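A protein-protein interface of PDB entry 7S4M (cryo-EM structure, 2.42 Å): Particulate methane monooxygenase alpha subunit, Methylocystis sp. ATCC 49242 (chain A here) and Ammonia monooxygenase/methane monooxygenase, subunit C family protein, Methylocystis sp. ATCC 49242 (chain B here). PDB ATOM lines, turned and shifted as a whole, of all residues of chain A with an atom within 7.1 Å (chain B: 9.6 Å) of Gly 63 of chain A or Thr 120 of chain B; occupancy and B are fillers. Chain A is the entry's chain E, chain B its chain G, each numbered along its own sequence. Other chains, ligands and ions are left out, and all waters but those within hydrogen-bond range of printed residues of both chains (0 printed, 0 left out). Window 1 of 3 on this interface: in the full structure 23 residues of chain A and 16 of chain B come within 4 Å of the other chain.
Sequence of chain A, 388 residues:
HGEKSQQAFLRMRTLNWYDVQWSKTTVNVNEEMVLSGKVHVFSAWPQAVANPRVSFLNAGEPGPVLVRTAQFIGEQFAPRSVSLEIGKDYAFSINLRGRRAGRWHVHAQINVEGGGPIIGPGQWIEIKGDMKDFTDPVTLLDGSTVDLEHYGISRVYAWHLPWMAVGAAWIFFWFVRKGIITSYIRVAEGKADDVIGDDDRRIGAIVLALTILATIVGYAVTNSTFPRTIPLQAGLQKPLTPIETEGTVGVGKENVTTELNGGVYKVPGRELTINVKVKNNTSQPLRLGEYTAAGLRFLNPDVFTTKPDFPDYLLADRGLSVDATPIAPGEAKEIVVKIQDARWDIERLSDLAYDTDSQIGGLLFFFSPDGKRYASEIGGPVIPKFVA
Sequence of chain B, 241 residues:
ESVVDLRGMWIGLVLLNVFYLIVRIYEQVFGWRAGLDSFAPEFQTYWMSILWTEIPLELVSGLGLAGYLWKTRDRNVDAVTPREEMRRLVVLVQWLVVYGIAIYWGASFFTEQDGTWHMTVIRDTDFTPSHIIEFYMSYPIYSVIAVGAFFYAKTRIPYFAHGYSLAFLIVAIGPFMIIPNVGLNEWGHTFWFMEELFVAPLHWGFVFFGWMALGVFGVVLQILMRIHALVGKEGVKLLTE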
ATOM      1  N   ALA A  59      30.673 -28.319 -28.509  1.00  0.00           N
ATOM      2  CA  ALA A  59      29.270 -28.159 -28.870  1.00  0.00           C
ATOM      3  C   ALA A  59      29.081 -26.752 -29.424  1.00  0.00           C
ATOM      4  O   ALA A  59      29.269 -25.767 -28.706  1.00  0.00           O
ATOM      5  CB  ALA A  59      28.364 -28.401 -27.667  1.00  0.00           C
ATOM      6  N   GLY A  60      28.708 -26.660 -30.696  1.00  0.00           N
ATOM      7  CA  GLY A  60      28.536 -25.368 -31.327  1.00  0.00           C
ATOM      8  C   GLY A  60      27.201 -24.736 -31.003  1.00  0.00           C
ATOM      9  O   GLY A  60      26.167 -25.152 -31.530  1.00  0.00           O
ATOM     10  N   GLU A  61      27.214 -23.729 -30.137  1.00  0.00           N
ATOM     11  CA  GLU A  61      25.997 -23.083 -29.675  1.00  0.00           C
ATOM     12  C   GLU A  61      26.287 -21.615 -29.427  1.00  0.00           C
ATOM     13  O   GLU A  61      27.437 -21.250 -29.161  1.00  0.00           O
ATOM     14  CB  GLU A  61      25.480 -23.745 -28.392  1.00  0.00           C
ATOM     15  CG  GLU A  61      26.573 -24.015 -27.388  1.00  0.00           C
ATOM     16  CD  GLU A  61      26.033 -24.400 -26.036  1.00  0.00           C
ATOM     17  OE1 GLU A  61      24.822 -24.224 -25.805  1.00  0.00           O
ATOM     18  OE2 GLU A  61      26.821 -24.879 -25.201  1.00  0.00           O
ATOM     19  N   PRO A  62      25.278 -20.752 -29.504  1.00  0.00           N
ATOM     20  CA  PRO A  62      25.513 -19.326 -29.245  1.00  0.00           C
ATOM     21  C   PRO A  62      25.724 -19.033 -27.771  1.00  0.00           C
ATOM     22  O   PRO A  62      24.804 -18.583 -27.080  1.00  0.00           O
ATOM     23  CB  PRO A  62      24.236 -18.664 -29.772  1.00  0.00           C
ATOM     24  CG  PRO A  62      23.199 -19.716 -29.643  1.00  0.00           C
ATOM     25  CD  PRO A  62      23.892 -21.014 -29.924  1.00  0.00           C
ATOM     26  N   GLY A  63      26.933 -19.277 -27.278  1.00  0.00           N
ATOM     27  CA  GLY A  63      27.236 -19.073 -25.884  1.00  0.00           C
ATOM     28  C   GLY A  63      26.782 -20.240 -25.035  1.00  0.00           C
ATOM     29  O   GLY A  63      26.317 -21.264 -25.544  1.00  0.00           O
ATOM     30  N   PRO A  64      26.911 -20.111 -23.726  1.00  0.00           N
ATOM     31  CA  PRO A  64      26.530 -21.184 -22.800  1.00  0.00           C
ATOM     32  C   PRO A  64      25.031 -21.242 -22.519  1.00  0.00           C
ATOM     33  O   PRO A  64      24.597 -21.236 -21.366  1.00  0.00           O
ATOM     34  CB  PRO A  64      27.328 -20.840 -21.541  1.00  0.00           C
ATOM     35  CG  PRO A  64      27.404 -19.364 -21.568  1.00  0.00           C
ATOM     36  CD  PRO A  64      27.493 -18.960 -23.018  1.00  0.00           C
ATOM     37  N   VAL A  65      24.231 -21.291 -23.584  1.00  0.00           N
ATOM     38  CA  VAL A  65      22.802 -21.514 -23.403  1.00  0.00           C
ATOM     39  C   VAL A  65      22.551 -22.932 -22.916  1.00  0.00           C
ATOM     40  O   VAL A  65      21.535 -23.206 -22.268  1.00  0.00           O
ATOM     41  CB  VAL A  65      22.034 -21.210 -24.701  1.00  0.00           C
ATOM     42  CG1 VAL A  65      22.245 -19.768 -25.109  1.00  0.00           C
ATOM     43  CG2 VAL A  65      22.471 -22.140 -25.809  1.00  0.00           C
ATOM     44  N   LEU A  66      23.460 -23.852 -23.218  1.00  0.00           N
ATOM     45  CA  LEU A  66      23.422 -25.213 -22.707  1.00  0.00           C
ATOM     46  C   LEU A  66      24.767 -25.533 -22.076  1.00  0.00           C
ATOM     47  O   LEU A  66      25.803 -25.436 -22.738  1.00  0.00           O
ATOM     48  CB  LEU A  66      23.104 -26.212 -23.820  1.00  0.00           C
ATOM     49  CG  LEU A  66      21.630 -26.378 -24.183  1.00  0.00           C
ATOM     50  CD1 LEU A  66      21.482 -26.588 -25.668  1.00  0.00           C
ATOM     51  CD2 LEU A  66      21.039 -27.548 -23.434  1.00  0.00           C
ATOM     52  N   VAL A  67      24.750 -25.914 -20.808  1.00  0.00           N
ATOM     53  CA  VAL A  67      25.973 -26.223 -20.079  1.00  0.00           C
ATOM     54  C   VAL A  67      26.383 -27.656 -20.380  1.00  0.00           C
ATOM     55  O   VAL A  67      25.572 -28.582 -20.271  1.00  0.00           O
ATOM     56  CB  VAL A  67      25.784 -26.005 -18.571  1.00  0.00           C
ATOM     57  CG1 VAL A  67      26.827 -26.772 -17.788  1.00  0.00           C
ATOM     58  CG2 VAL A  67      25.883 -24.533 -18.259  1.00  0.00           C
ATOM     59  N   ARG A  99      20.185 -24.197 -19.880  1.00  0.00           N
ATOM     60  CA  ARG A  99      20.490 -23.075 -19.002  1.00  0.00           C
ATOM     61  C   ARG A  99      19.708 -21.813 -19.328  1.00  0.00           C
ATOM     62  O   ARG A  99      19.256 -21.126 -18.410  1.00  0.00           O
ATOM     63  CB  ARG A  99      21.990 -22.769 -19.055  1.00  0.00           C
ATOM     64  CG  ARG A  99      22.398 -21.569 -18.231  1.00  0.00           C
ATOM     65  CD  ARG A  99      23.885 -21.562 -17.972  1.00  0.00           C
ATOM     66  NE  ARG A  99      24.298 -20.372 -17.241  1.00  0.00           N
ATOM     67  CZ  ARG A  99      24.858 -19.312 -17.805  1.00  0.00           C
ATOM     68  NH1 ARG A  99      25.090 -19.263 -19.104  1.00  0.00           N
ATOM     69  NH2 ARG A  99      25.194 -18.276 -17.043  1.00  0.00           N
ATOM     70  N   ARG A 100      19.529 -21.491 -20.604  1.00  0.00           N
ATOM     71  CA  ARG A 100      18.914 -20.238 -21.014  1.00  0.00           C
ATOM     72  C   ARG A 100      17.680 -20.519 -21.855  1.00  0.00           C
ATOM     73  O   ARG A 100      17.750 -21.270 -22.832  1.00  0.00           O
ATOM     74  CB  ARG A 100      19.896 -19.379 -21.807  1.00  0.00           C
ATOM     75  CG  ARG A 100      20.564 -18.298 -20.991  1.00  0.00           C
ATOM     76  CD  ARG A 100      21.325 -17.337 -21.879  1.00  0.00           C
ATOM     77  NE  ARG A 100      20.427 -16.464 -22.624  1.00  0.00           N
ATOM     78  CZ  ARG A 100      20.748 -15.855 -23.756  1.00  0.00           C
ATOM     79  NH1 ARG A 100      21.942 -16.000 -24.304  1.00  0.00           N
ATOM     80  NH2 ARG A 100      19.849 -15.075 -24.349  1.00  0.00           N
ATOM     81  N   GLY B  31      21.439  -8.985 -30.560  1.00  0.00           N
ATOM     82  CA  GLY B  31      22.590  -9.860 -30.714  1.00  0.00           C
ATOM     83  C   GLY B  31      22.166 -11.273 -31.055  1.00  0.00           C
ATOM     84  O   GLY B  31      22.737 -11.917 -31.938  1.00  0.00           O
ATOM     85  N   TRP B  32      21.166 -11.773 -30.347  1.00  0.00           N
ATOM     86  CA  TRP B  32      20.357 -12.889 -30.798  1.00  0.00           C
ATOM     87  C   TRP B  32      19.119 -12.321 -31.466  1.00  0.00           C
ATOM     88  O   TRP B  32      18.901 -11.108 -31.471  1.00  0.00           O
ATOM     89  CB  TRP B  32      19.987 -13.796 -29.628  1.00  0.00           C
ATOM     90  CG  TRP B  32      21.180 -14.190 -28.826  1.00  0.00           C
ATOM     91  CD1 TRP B  32      21.870 -15.363 -28.903  1.00  0.00           C
ATOM     92  CD2 TRP B  32      21.849 -13.395 -27.845  1.00  0.00           C
ATOM     93  NE1 TRP B  32      22.920 -15.353 -28.021  1.00  0.00           N
ATOM     94  CE2 TRP B  32      22.928 -14.155 -27.359  1.00  0.00           C
ATOM     95  CE3 TRP B  32      21.634 -12.117 -27.326  1.00  0.00           C
ATOM     96  CZ2 TRP B  32      23.789 -13.679 -26.383  1.00  0.00           C
ATOM     97  CZ3 TRP B  32      22.488 -11.649 -26.361  1.00  0.00           C
ATOM     98  CH2 TRP B  32      23.553 -12.424 -25.900  1.00  0.00           C
ATOM     99  N   GLY B  35      20.795 -11.518 -34.953  1.00  0.00           N
ATOM    100  CA  GLY B  35      22.157 -11.037 -34.851  1.00  0.00           C
ATOM    101  C   GLY B  35      23.203 -12.128 -34.963  1.00  0.00           C
ATOM    102  O   GLY B  35      24.401 -11.840 -35.006  1.00  0.00           O
ATOM    103  N   LEU B  36      22.767 -13.389 -34.972  1.00  0.00           N
ATOM    104  CA  LEU B  36      23.738 -14.516 -34.990  1.00  0.00           C
ATOM    105  C   LEU B  36      24.104 -14.863 -36.437  1.00  0.00           C
ATOM    106  O   LEU B  36      25.303 -14.780 -36.770  1.00  0.00           O
ATOM    107  CB  LEU B  36      23.113 -15.715 -34.276  1.00  0.00           C
ATOM    108  CG  LEU B  36      22.772 -15.499 -32.804  1.00  0.00           C
ATOM    109  CD1 LEU B  36      21.877 -16.617 -32.295  1.00  0.00           C
ATOM    110  CD2 LEU B  36      24.037 -15.402 -31.965  1.00  0.00           C
ATOM    111  N   ASP B  37      23.116 -15.238 -37.256  1.00  0.00           N
ATOM    112  CA  ASP B  37      23.401 -15.662 -38.654  1.00  0.00           C
ATOM    113  C   ASP B  37      23.512 -14.439 -39.561  1.00  0.00           C
ATOM    114  O   ASP B  37      22.533 -13.681 -39.636  1.00  0.00           O
ATOM    115  CB  ASP B  37      22.358 -16.645 -39.182  1.00  0.00           C
ATOM    116  CG  ASP B  37      22.817 -17.337 -40.453  1.00  0.00           C
ATOM    117  OD1 ASP B  37      23.608 -18.290 -40.349  1.00  0.00           O
ATOM    118  OD2 ASP B  37      22.389 -16.905 -41.536  1.00  0.00           O
ATOM    119  N   GLN B 113      34.409  -6.102 -25.870  1.00  0.00           N
ATOM    120  CA  GLN B 113      33.135  -6.769 -26.109  1.00  0.00           C
ATOM    121  C   GLN B 113      33.229  -7.701 -27.308  1.00  0.00           C
ATOM    122  O   GLN B 113      32.627  -8.782 -27.311  1.00  0.00           O
ATOM    123  CB  GLN B 113      32.033  -5.734 -26.320  1.00  0.00           C
ATOM    124  CG  GLN B 113      30.674  -6.336 -26.583  1.00  0.00           C
ATOM    125  CD  GLN B 113      29.664  -5.309 -27.034  1.00  0.00           C
ATOM    126  OE1 GLN B 113      29.639  -4.918 -28.198  1.00  0.00           O
ATOM    127  NE2 GLN B 113      28.820  -4.867 -26.111  1.00  0.00           N
ATOM    128  N   ASP B 114      33.979  -7.294 -28.333  1.00  0.00           N
ATOM    129  CA  ASP B 114      34.284  -8.203 -29.430  1.00  0.00           C
ATOM    130  C   ASP B 114      34.942  -9.479 -28.929  1.00  0.00           C
ATOM    131  O   ASP B 114      34.790 -10.539 -29.544  1.00  0.00           O
ATOM    132  CB  ASP B 114      35.184  -7.517 -30.454  1.00  0.00           C
ATOM    133  CG  ASP B 114      35.254  -8.273 -31.763  1.00  0.00           C
ATOM    134  OD1 ASP B 114      34.233  -8.872 -32.155  1.00  0.00           O
ATOM    135  OD2 ASP B 114      36.328  -8.271 -32.397  1.00  0.00           O
ATOM    136  N   GLY B 115      35.677  -9.396 -27.820  1.00  0.00           N
ATOM    137  CA  GLY B 115      36.268 -10.594 -27.251  1.00  0.00           C
ATOM    138  C   GLY B 115      35.230 -11.595 -26.788  1.00  0.00           C
ATOM    139  O   GLY B 115      35.346 -12.792 -27.062  1.00  0.00           O
ATOM    140  N   THR B 116      34.200 -11.125 -26.082  1.00  0.00           N
ATOM    141  CA  THR B 116      33.171 -12.045 -25.615  1.00  0.00           C
ATOM    142  C   THR B 116      32.248 -12.473 -26.746  1.00  0.00           C
ATOM    143  O   THR B 116      31.673 -13.565 -26.690  1.00  0.00           O
ATOM    144  CB  THR B 116      32.372 -11.421 -24.469  1.00  0.00           C
ATOM    145  OG1 THR B 116      31.677 -12.453 -23.758  1.00  0.00           O
ATOM    146  CG2 THR B 116      31.360 -10.419 -24.981  1.00  0.00           C
ATOM    147  N   TRP B 117      32.097 -11.645 -27.782  1.00  0.00           N
ATOM    148  CA  TRP B 117      31.292 -12.074 -28.920  1.00  0.00           C
ATOM    149  C   TRP B 117      31.988 -13.169 -29.712  1.00  0.00           C
ATOM    150  O   TRP B 117      31.319 -14.022 -30.304  1.00  0.00           O
ATOM    151  CB  TRP B 117      30.971 -10.895 -29.831  1.00  0.00           C
ATOM    152  CG  TRP B 117      29.961 -11.233 -30.881  1.00  0.00           C
ATOM    153  CD1 TRP B 117      30.176 -11.329 -32.223  1.00  0.00           C
ATOM    154  CD2 TRP B 117      28.577 -11.534 -30.675  1.00  0.00           C
ATOM    155  NE1 TRP B 117      29.010 -11.663 -32.867  1.00  0.00           N
ATOM    156  CE2 TRP B 117      28.014 -11.795 -31.938  1.00  0.00           C
ATOM    157  CE3 TRP B 117      27.759 -11.605 -29.546  1.00  0.00           C
ATOM    158  CZ2 TRP B 117      26.673 -12.120 -32.102  1.00  0.00           C
ATOM    159  CZ3 TRP B 117      26.428 -11.926 -29.711  1.00  0.00           C
ATOM    160  CH2 TRP B 117      25.898 -12.182 -30.979  1.00  0.00           C
ATOM    161  N   HIS B 118      33.320 -13.163 -29.737  1.00  0.00           N
ATOM    162  CA  HIS B 118      34.051 -14.189 -30.466  1.00  0.00           C
ATOM    163  C   HIS B 118      33.873 -15.570 -29.858  1.00  0.00           C
ATOM    164  O   HIS B 118      34.073 -16.568 -30.556  1.00  0.00           O
ATOM    165  CB  HIS B 118      35.533 -13.832 -30.524  1.00  0.00           C
ATOM    166  CG  HIS B 118      35.848 -12.731 -31.485  1.00  0.00           C
ATOM    167  ND1 HIS B 118      35.070 -12.465 -32.591  1.00  0.00           N
ATOM    168  CD2 HIS B 118      36.853 -11.825 -31.506  1.00  0.00           C
ATOM    169  CE1 HIS B 118      35.583 -11.444 -33.252  1.00  0.00           C
ATOM    170  NE2 HIS B 118      36.666 -11.037 -32.615  1.00  0.00           N
ATOM    171  N   MET B 119      33.502 -15.655 -28.585  1.00  0.00           N
ATOM    172  CA  MET B 119      33.245 -16.933 -27.939  1.00  0.00           C
ATOM    173  C   MET B 119      31.789 -17.355 -28.035  1.00  0.00           C
ATOM    174  O   MET B 119      31.445 -18.451 -27.585  1.00  0.00           O
ATOM    175  CB  MET B 119      33.668 -16.877 -26.472  1.00  0.00           C
ATOM    176  CG  MET B 119      35.166 -16.923 -26.270  1.00  0.00           C
ATOM    177  SD  MET B 119      36.029 -17.691 -27.648  1.00  0.00           S
ATOM    178  CE  MET B 119      37.528 -16.716 -27.682  1.00  0.00           C
ATOM    179  N   THR B 120      30.933 -16.519 -28.614  1.00  0.00           N
ATOM    180  CA  THR B 120      29.526 -16.836 -28.800  1.00  0.00           C
ATOM    181  C   THR B 120      29.202 -17.331 -30.196  1.00  0.00           C
ATOM    182  O   THR B 120      28.325 -18.183 -30.348  1.00  0.00           O
ATOM    183  CB  THR B 120      28.664 -15.604 -28.501  1.00  0.00           C
ATOM    184  OG1 THR B 120      29.097 -15.010 -27.273  1.00  0.00           O
ATOM    185  CG2 THR B 120      27.203 -15.984 -28.381  1.00  0.00           C
ATOM    186  N   VAL B 121      29.896 -16.831 -31.212  1.00  0.00           N
ATOM    187  CA  VAL B 121      29.669 -17.231 -32.590  1.00  0.00           C
ATOM    188  C   VAL B 121      30.945 -17.864 -33.126  1.00  0.00           C
ATOM    189  O   VAL B 121      32.007 -17.801 -32.511  1.00  0.00           O
ATOM    190  CB  VAL B 121      29.236 -16.051 -33.477  1.00  0.00           C
ATOM    191  CG1 VAL B 121      28.051 -15.336 -32.859  1.00  0.00           C
ATOM    192  CG2 VAL B 121      30.395 -15.094 -33.678  1.00  0.00           C
ATOM    193  N   ILE B 122      30.820 -18.481 -34.294  1.00  0.00           N
ATOM    194  CA  ILE B 122      31.954 -19.067 -34.985  1.00  0.00           C
ATOM    195  C   ILE B 122      32.431 -18.161 -36.123  1.00  0.00           C
ATOM    196  O   ILE B 122      33.022 -18.635 -37.092  1.00  0.00           O
ATOM    197  CB  ILE B 122      31.631 -20.483 -35.480  1.00  0.00           C
ATOM    198  CG1 ILE B 122      30.781 -21.203 -34.438  1.00  0.00           C
ATOM    199  CG2 ILE B 122      32.901 -21.287 -35.671  1.00  0.00           C
ATOM    200  CD1 ILE B 122      30.349 -22.586 -34.846  1.00  0.00           C
ATOM    201  N   ARG B 123      32.170 -16.856 -36.017  1.00  0.00           N
ATOM    202  CA  ARG B 123      32.620 -15.854 -36.980  1.00  0.00           C
ATOM    203  C   ARG B 123      32.073 -16.147 -38.379  1.00  0.00           C
ATOM    204  O   ARG B 123      32.797 -16.497 -39.310  1.00  0.00           O
ATOM    205  CB  ARG B 123      34.149 -15.753 -36.988  1.00  0.00           C
ATOM    206  CG  ARG B 123      34.737 -15.405 -35.638  1.00  0.00           C
ATOM    207  CD  ARG B 123      35.819 -14.362 -35.786  1.00  0.00           C
ATOM    208  NE  ARG B 123      35.333 -13.207 -36.530  1.00  0.00           N
ATOM    209  CZ  ARG B 123      35.740 -12.878 -37.746  1.00  0.00           C
ATOM    210  NH1 ARG B 123      36.661 -13.584 -38.381  1.00  0.00           N
ATOM    211  NH2 ARG B 123      35.206 -11.817 -38.343  1.00  0.00           N
ATOM    212  N   ASP B 124      30.748 -16.016 -38.486  1.00  0.00           N
ATOM    213  CA  ASP B 124      30.085 -16.195 -39.773  1.00  0.00           C
ATOM    214  C   ASP B 124      30.657 -15.270 -40.841  1.00  0.00           C
ATOM    215  O   ASP B 124      30.716 -15.645 -42.017  1.00  0.00           O
ATOM    216  CB  ASP B 124      28.580 -15.960 -39.622  1.00  0.00           C
ATOM    217  CG  ASP B 124      27.769 -16.636 -40.711  1.00  0.00           C
ATOM    218  OD1 ASP B 124      28.373 -17.176 -41.662  1.00  0.00           O
ATOM    219  OD2 ASP B 124      26.523 -16.623 -40.617  1.00  0.00           O
ATOM    220  N   THR B 128      30.400  -8.872 -38.119  1.00  0.00           N
ATOM    221  CA  THR B 128      29.612  -9.292 -36.976  1.00  0.00           C
ATOM    222  C   THR B 128      29.013  -8.077 -36.280  1.00  0.00           C
ATOM    223  O   THR B 128      29.489  -6.954 -36.460  1.00  0.00           O
ATOM    224  CB  THR B 128      30.474 -10.080 -35.997  1.00  0.00           C
ATOM    225  OG1 THR B 128      31.383  -9.190 -35.340  1.00  0.00           O
ATOM    226  CG2 THR B 128      31.260 -11.149 -36.727  1.00  0.00           C
ATOM    227  N   PRO B 129      27.950  -8.269 -35.496  1.00  0.00           N
ATOM    228  CA  PRO B 129      27.403  -7.138 -34.729  1.00  0.00           C
ATOM    229  C   PRO B 129      28.445  -6.434 -33.880  1.00  0.00           C
ATOM    230  O   PRO B 129      28.477  -5.199 -33.841  1.00  0.00           O
ATOM    231  CB  PRO B 129      26.320  -7.788 -33.857  1.00  0.00           C
ATOM    232  CG  PRO B 129      26.104  -9.159 -34.398  1.00  0.00           C
ATOM    233  CD  PRO B 129      27.035  -9.419 -35.532  1.00  0.00           C
ATOM    234  N   SER B 130      29.316  -7.191 -33.213  1.00  0.00           N
ATOM    235  CA  SER B 130      30.379  -6.572 -32.434  1.00  0.00           C
ATOM    236  C   SER B 130      31.327  -5.786 -33.328  1.00  0.00           C
ATOM    237  O   SER B 130      31.731  -4.670 -32.983  1.00  0.00           O
ATOM    238  CB  SER B 130      31.141  -7.636 -31.650  1.00  0.00           C
ATOM    239  OG  SER B 130      32.135  -8.237 -32.459  1.00  0.00           O
ATOM    240  N   GLU B 196      40.816 -18.186 -32.246  1.00  0.00           N
ATOM    241  CA  GLU B 196      40.477 -16.872 -31.706  1.00  0.00           C
ATOM    242  C   GLU B 196      41.353 -16.555 -30.491  1.00  0.00           C
ATOM    243  O   GLU B 196      40.894 -16.430 -29.358  1.00  0.00           O
ATOM    244  CB  GLU B 196      38.998 -16.813 -31.356  1.00  0.00           C
ATOM    245  CG  GLU B 196      38.298 -15.593 -31.909  1.00  0.00           C
ATOM    246  CD  GLU B 196      37.950 -15.743 -33.373  1.00  0.00           C
ATOM    247  OE1 GLU B 196      37.085 -16.584 -33.697  1.00  0.00           O
ATOM    248  OE2 GLU B 196      38.544 -15.022 -34.202  1.00  0.00           O
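O of Glu 61 of chain A sits close to O of Thr 120 of chain B.
The backbone NH (N) of Leu 66 of chain A sits at hydrogen-bond distance from the side-chain carboxylate (OE1) of Glu 61 of chain A.
N of Arg 100 of chain A is in hydrogen-bond range of O of Val 65 of chain A, at 3.1 Å.
N of Leu 36 of chain B lies within hydrogen-bond range of O of Gly 31 of chain B (3.4 Å).
The side-chain hydroxyl of Thr 120 of chain B lies within hydrogen-bond range of the backbone carbonyl oxygen of Thr 116 of chain B.
Trp 32 of chain B touches Pro 62 of chain A.
Leu 36 of chain B touches Pro 62 of chain A.
Thr 120 of chain B touches Pro 62 of chain A (O to CA, 3.2 Å).
Thr 120 of chain B touches Gly 63 of chain A.
Arg 100 of chain A touches Trp 32 of chain B (NH1 to CZ2, 3.6 Å).
Of chain B, only Thr 120 (3.4 Å) comes within 4 Å of Glu 61 of chain A.
No residue of chain B comes within 4 Å of Pro 64 of chain A.
Of the printed residues of chain B, Arg 100 of chain A touches Trp 32.
Printed residues of chain A within 4 Å of Trp 32 of chain B: Pro 62 (3.9 Å) and Arg 100 (3.6 Å).
Of the printed residues of chain A, Leu 36 of chain B touches Pro 62 (3.9 Å).
Gln 113 of chain B touches none of the printed residues of chain A.
Of chain A, only Glu 61 (3.4 Å), Pro 62 (3.2 Å) and Gly 63 (3.5 Å) come within 4 Å of Thr 120 of chain B.
Ser 130 of chain B touches none of the printed residues of chain A.
The nearest printed residue of chain B that does not touch Arg 100 of chain A is Thr 120 of chain B (6.7 Å).
Printed residues of chain B that touch a printed residue of chain A: Trp 32, Leu 36 and Thr 120.
Hydrophobic or aromatic side chains of chain B within 4 Å of the printed part of chain A: Trp 32 and Leu 36.
Printed residues of chain A that touch a printed residue of chain B: Glu 61, Pro 62, Gly 63 and Arg 100.
Hydrophobic or aromatic side chains of chain A within 4 Å of the printed part of chain B: Pro 62.
Among the printed residues, 6 pairs touch across the chains.
Among the printed residues, no Asp or Glu carboxylate lies within 4 Å of a Lys or Arg side-chain nitrogen of the other chain.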
